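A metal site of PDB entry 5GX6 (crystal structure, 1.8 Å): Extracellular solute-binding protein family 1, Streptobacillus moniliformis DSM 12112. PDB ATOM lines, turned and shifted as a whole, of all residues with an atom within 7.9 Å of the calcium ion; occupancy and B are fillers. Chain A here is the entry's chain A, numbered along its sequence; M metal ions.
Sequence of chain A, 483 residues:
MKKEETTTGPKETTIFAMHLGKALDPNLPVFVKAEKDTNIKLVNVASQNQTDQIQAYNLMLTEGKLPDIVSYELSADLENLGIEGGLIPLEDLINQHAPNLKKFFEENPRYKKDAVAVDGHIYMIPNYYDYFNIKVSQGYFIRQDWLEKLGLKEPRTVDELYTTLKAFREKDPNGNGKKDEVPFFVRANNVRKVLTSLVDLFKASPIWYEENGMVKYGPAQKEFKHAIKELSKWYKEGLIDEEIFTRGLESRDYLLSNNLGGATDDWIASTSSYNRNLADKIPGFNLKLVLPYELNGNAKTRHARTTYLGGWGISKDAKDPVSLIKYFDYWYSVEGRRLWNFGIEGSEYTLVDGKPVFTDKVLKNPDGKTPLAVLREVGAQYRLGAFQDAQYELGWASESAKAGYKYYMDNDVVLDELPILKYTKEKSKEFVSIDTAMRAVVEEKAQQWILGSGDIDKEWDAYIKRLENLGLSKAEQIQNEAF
The calcium ion is bound by the side-chain amide oxygen (OD1) of Asn 174 (2.3 Å), the side-chain carboxylate (OD1) of Asp 172 (2.3 Å), the side-chain carboxylate (OD1) of Asp 180 (2.4 Å), the backbone carbonyl oxygen (O) of Lys 178 (2.4 Å), the side-chain carboxylate (OE2) of Glu 181 (2.5 Å), the side-chain amide oxygen (OD1) of Asn 176 (2.5 Å) and the side-chain carboxylate (OE1) of Glu 181 (2.7 Å).
The calcium ion has seven donor atoms within binding distance.
Of the 17 residues printed, 6 come within 4 Å of the calcium ion.
The backbone carbonyl oxygen of Asn 259 lies within hydrogen-bond range of the side-chain amide nitrogen of Asn 174 (2.9 Å).
The backbone NH of Gly 177 sits at hydrogen-bond distance from the side-chain carboxylate of Asp 172 (2.7 Å).
O of Glu 181 is in hydrogen-bond range of NH1 of Arg 169 (2.8 Å).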
ATOM      1  N   TRP A 146       6.336  11.469  -7.165  1.00  0.00           N
ATOM      2  CA  TRP A 146       5.457  12.592  -6.851  1.00  0.00           C
ATOM      3  C   TRP A 146       4.555  12.935  -8.038  1.00  0.00           C
ATOM      4  O   TRP A 146       3.397  13.318  -7.837  1.00  0.00           O
ATOM      5  CB  TRP A 146       6.290  13.808  -6.423  1.00  0.00           C
ATOM      6  CG  TRP A 146       6.816  13.702  -5.015  1.00  0.00           C
ATOM      7  CD1 TRP A 146       6.721  12.624  -4.170  1.00  0.00           C
ATOM      8  CD2 TRP A 146       7.521  14.715  -4.292  1.00  0.00           C
ATOM      9  NE1 TRP A 146       7.315  12.913  -2.964  1.00  0.00           N
ATOM     10  CE2 TRP A 146       7.821  14.191  -3.015  1.00  0.00           C
ATOM     11  CE3 TRP A 146       7.925  16.016  -4.595  1.00  0.00           C
ATOM     12  CZ2 TRP A 146       8.502  14.923  -2.047  1.00  0.00           C
ATOM     13  CZ3 TRP A 146       8.606  16.748  -3.626  1.00  0.00           C
ATOM     14  CH2 TRP A 146       8.889  16.194  -2.373  1.00  0.00           C
ATOM     15  N   PHE A 168       3.847  20.642  -6.819  1.00  0.00           N
ATOM     16  CA  PHE A 168       4.669  20.087  -5.746  1.00  0.00           C
ATOM     17  C   PHE A 168       4.591  20.949  -4.487  1.00  0.00           C
ATOM     18  O   PHE A 168       4.543  20.431  -3.371  1.00  0.00           O
ATOM     19  CB  PHE A 168       6.123  19.949  -6.192  1.00  0.00           C
ATOM     20  CG  PHE A 168       6.385  18.803  -7.154  1.00  0.00           C
ATOM     21  CD1 PHE A 168       5.378  17.940  -7.534  1.00  0.00           C
ATOM     22  CD2 PHE A 168       7.673  18.604  -7.654  1.00  0.00           C
ATOM     23  CE1 PHE A 168       5.639  16.884  -8.412  1.00  0.00           C
ATOM     24  CE2 PHE A 168       7.944  17.550  -8.533  1.00  0.00           C
ATOM     25  CZ  PHE A 168       6.916  16.692  -8.910  1.00  0.00           C
ATOM     26  N   ARG A 169       4.562  22.267  -4.657  1.00  0.00           N
ATOM     27  CA  ARG A 169       4.574  23.151  -3.504  1.00  0.00           C
ATOM     28  C   ARG A 169       3.228  23.184  -2.800  1.00  0.00           C
ATOM     29  O   ARG A 169       3.164  23.231  -1.570  1.00  0.00           O
ATOM     30  CB  ARG A 169       4.991  24.566  -3.924  1.00  0.00           C
ATOM     31  CG  ARG A 169       5.019  25.579  -2.784  1.00  0.00           C
ATOM     32  CD  ARG A 169       6.048  25.226  -1.721  1.00  0.00           C
ATOM     33  NE  ARG A 169       6.040  26.200  -0.635  1.00  0.00           N
ATOM     34  CZ  ARG A 169       6.597  26.021   0.557  1.00  0.00           C
ATOM     35  NH1 ARG A 169       7.212  24.878   0.852  1.00  0.00           N
ATOM     36  NH2 ARG A 169       6.518  26.981   1.465  1.00  0.00           N
ATOM     37  N   LYS A 171       0.348  20.979  -3.187  1.00  0.00           N
ATOM     38  CA  LYS A 171      -0.520  19.805  -3.087  1.00  0.00           C
ATOM     39  C   LYS A 171       0.079  18.657  -2.274  1.00  0.00           C
ATOM     40  O   LYS A 171      -0.342  17.510  -2.433  1.00  0.00           O
ATOM     41  CB  LYS A 171      -0.940  19.340  -4.476  1.00  0.00           C
ATOM     42  CG  LYS A 171      -1.760  20.386  -5.214  1.00  0.00           C
ATOM     43  CD  LYS A 171      -2.131  19.930  -6.606  1.00  0.00           C
ATOM     44  CE  LYS A 171      -3.583  20.235  -6.938  1.00  0.00           C
ATOM     45  NZ  LYS A 171      -3.948  19.656  -8.258  1.00  0.00           N
ATOM     46  N   ASP A 172       1.069  18.939  -1.429  1.00  0.00           N
ATOM     47  CA  ASP A 172       1.541  17.994  -0.412  1.00  0.00           C
ATOM     48  C   ASP A 172       1.920  16.622  -0.992  1.00  0.00           C
ATOM     49  O   ASP A 172       1.386  15.589  -0.516  1.00  0.00           O
ATOM     50  CB  ASP A 172       0.496  17.852   0.676  1.00  0.00           C
ATOM     51  CG  ASP A 172       1.001  17.067   1.876  1.00  0.00           C
ATOM     52  OD1 ASP A 172       2.193  17.187   2.222  1.00  0.00           O
ATOM     53  OD2 ASP A 172       0.200  16.309   2.466  1.00  0.00           O
ATOM     54  N   PRO A 173       2.789  16.541  -1.975  1.00  0.00           N
ATOM     55  CA  PRO A 173       3.136  15.233  -2.542  1.00  0.00           C
ATOM     56  C   PRO A 173       3.819  14.298  -1.553  1.00  0.00           C
ATOM     57  O   PRO A 173       3.745  13.089  -1.723  1.00  0.00           O
ATOM     58  CB  PRO A 173       4.057  15.575  -3.732  1.00  0.00           C
ATOM     59  CG  PRO A 173       4.609  16.901  -3.395  1.00  0.00           C
ATOM     60  CD  PRO A 173       3.513  17.631  -2.662  1.00  0.00           C
ATOM     61  N   ASN A 174       4.481  14.768  -0.509  1.00  0.00           N
ATOM     62  CA  ASN A 174       5.039  13.764   0.390  1.00  0.00           C
ATOM     63  C   ASN A 174       4.036  13.317   1.440  1.00  0.00           C
ATOM     64  O   ASN A 174       4.391  12.518   2.316  1.00  0.00           O
ATOM     65  CB  ASN A 174       6.356  14.240   1.020  1.00  0.00           C
ATOM     66  CG  ASN A 174       6.204  15.404   1.985  1.00  0.00           C
ATOM     67  OD1 ASN A 174       5.102  15.774   2.392  1.00  0.00           O
ATOM     68  ND2 ASN A 174       7.334  15.981   2.363  1.00  0.00           N
ATOM     69  N   GLY A 175       2.809  13.830   1.402  1.00  0.00           N
ATOM     70  CA  GLY A 175       1.686  13.247   2.088  1.00  0.00           C
ATOM     71  C   GLY A 175       1.591  13.504   3.575  1.00  0.00           C
ATOM     72  O   GLY A 175       0.786  12.845   4.241  1.00  0.00           O
ATOM     73  N   ASN A 176       2.383  14.426   4.125  1.00  0.00           N
ATOM     74  CA  ASN A 176       2.403  14.648   5.566  1.00  0.00           C
ATOM     75  C   ASN A 176       1.542  15.825   6.008  1.00  0.00           C
ATOM     76  O   ASN A 176       1.639  16.252   7.158  1.00  0.00           O
ATOM     77  CB  ASN A 176       3.841  14.808   6.058  1.00  0.00           C
ATOM     78  CG  ASN A 176       4.548  16.023   5.472  1.00  0.00           C
ATOM     79  OD1 ASN A 176       3.943  16.876   4.819  1.00  0.00           O
ATOM     80  ND2 ASN A 176       5.852  16.107   5.711  1.00  0.00           N
ATOM     81  N   GLY A 177       0.695  16.357   5.117  1.00  0.00           N
ATOM     82  CA  GLY A 177      -0.169  17.466   5.469  1.00  0.00           C
ATOM     83  C   GLY A 177       0.528  18.770   5.779  1.00  0.00           C
ATOM     84  O   GLY A 177      -0.096  19.686   6.304  1.00  0.00           O
ATOM     85  N   LYS A 178       1.822  18.882   5.455  1.00  0.00           N
ATOM     86  CA  LYS A 178       2.608  20.074   5.731  1.00  0.00           C
ATOM     87  C   LYS A 178       3.076  20.676   4.417  1.00  0.00           C
ATOM     88  O   LYS A 178       3.405  19.949   3.479  1.00  0.00           O
ATOM     89  CB  LYS A 178       3.806  19.723   6.576  1.00  0.00           C
ATOM     90  CG  LYS A 178       3.381  19.168   7.903  1.00  0.00           C
ATOM     91  CD  LYS A 178       4.530  18.482   8.612  1.00  0.00           C
ATOM     92  CE  LYS A 178       5.265  19.359   9.567  1.00  0.00           C
ATOM     93  NZ  LYS A 178       4.411  19.383  10.794  1.00  0.00           N
ATOM     94  N   LYS A 179       3.125  21.998   4.362  1.00  0.00           N
ATOM     95  CA  LYS A 179       3.655  22.708   3.210  1.00  0.00           C
ATOM     96  C   LYS A 179       5.169  22.849   3.389  1.00  0.00           C
ATOM     97  O   LYS A 179       5.708  23.932   3.630  1.00  0.00           O
ATOM     98  CB  LYS A 179       2.951  24.050   3.054  1.00  0.00           C
ATOM     99  CG  LYS A 179       3.186  24.754   1.745  1.00  0.00           C
ATOM    100  CD  LYS A 179       2.637  26.160   1.807  1.00  0.00           C
ATOM    101  CE  LYS A 179       2.613  26.818   0.444  1.00  0.00           C
ATOM    102  NZ  LYS A 179       2.030  28.192   0.535  1.00  0.00           N
ATOM    103  N   ASP A 180       5.850  21.710   3.283  1.00  0.00           N
ATOM    104  CA  ASP A 180       7.294  21.637   3.507  1.00  0.00           C
ATOM    105  C   ASP A 180       8.066  21.319   2.234  1.00  0.00           C
ATOM    106  O   ASP A 180       9.307  21.290   2.280  1.00  0.00           O
ATOM    107  CB  ASP A 180       7.613  20.611   4.597  1.00  0.00           C
ATOM    108  CG  ASP A 180       7.159  19.191   4.248  1.00  0.00           C
ATOM    109  OD1 ASP A 180       6.358  19.009   3.309  1.00  0.00           O
ATOM    110  OD2 ASP A 180       7.599  18.252   4.933  1.00  0.00           O
ATOM    111  N   GLU A 181       7.385  21.093   1.116  1.00  0.00           N
ATOM    112  CA  GLU A 181       8.053  20.690  -0.119  1.00  0.00           C
ATOM    113  C   GLU A 181       8.958  21.787  -0.660  1.00  0.00           C
ATOM    114  O   GLU A 181       8.599  22.966  -0.648  1.00  0.00           O
ATOM    115  CB  GLU A 181       7.008  20.308  -1.166  1.00  0.00           C
ATOM    116  CG  GLU A 181       6.486  18.870  -1.035  1.00  0.00           C
ATOM    117  CD  GLU A 181       5.422  18.707   0.042  1.00  0.00           C
ATOM    118  OE1 GLU A 181       5.003  19.705   0.662  1.00  0.00           O
ATOM    119  OE2 GLU A 181       4.996  17.551   0.246  1.00  0.00           O
ATOM    120  N   VAL A 182      10.132  21.388  -1.128  1.00  0.00           N
ATOM    121  CA  VAL A 182      11.069  22.260  -1.826  1.00  0.00           C
ATOM    122  C   VAL A 182      11.094  21.789  -3.277  1.00  0.00           C
ATOM    123  O   VAL A 182      11.820  20.836  -3.593  1.00  0.00           O
ATOM    124  CB  VAL A 182      12.462  22.222  -1.176  1.00  0.00           C
ATOM    125  CG1 VAL A 182      13.440  23.114  -1.956  1.00  0.00           C
ATOM    126  CG2 VAL A 182      12.375  22.692   0.270  1.00  0.00           C
ATOM    127  N   ASN A 259      12.943  13.805   2.260  1.00  0.00           N
ATOM    128  CA  ASN A 259      11.764  13.711   1.388  1.00  0.00           C
ATOM    129  C   ASN A 259      11.112  15.074   1.159  1.00  0.00           C
ATOM    130  O   ASN A 259       9.885  15.210   1.158  1.00  0.00           O
ATOM    131  CB  ASN A 259      10.751  12.706   1.942  1.00  0.00           C
ATOM    132  CG  ASN A 259       9.815  12.170   0.883  1.00  0.00           C
ATOM    133  OD1 ASN A 259      10.096  12.278  -0.314  1.00  0.00           O
ATOM    134  ND2 ASN A 259       8.697  11.586   1.324  1.00  0.00           N
ATOM    135  N   LEU A 260      11.939  16.102   0.961  1.00  0.00           N
ATOM    136  CA  LEU A 260      11.471  17.458   0.714  1.00  0.00           C
ATOM    137  C   LEU A 260      11.650  17.928  -0.725  1.00  0.00           C
ATOM    138  O   LEU A 260      10.842  18.718  -1.207  1.00  0.00           O
ATOM    139  CB  LEU A 260      12.213  18.446   1.633  1.00  0.00           C
ATOM    140  CG  LEU A 260      12.155  18.232   3.149  1.00  0.00           C
ATOM    141  CD1 LEU A 260      13.007  19.273   3.854  1.00  0.00           C
ATOM    142  CD2 LEU A 260      10.710  18.282   3.642  1.00  0.00           C
HETATM  143 CA    CA M   1       4.349  17.943   2.594  1.00  0.00          CA
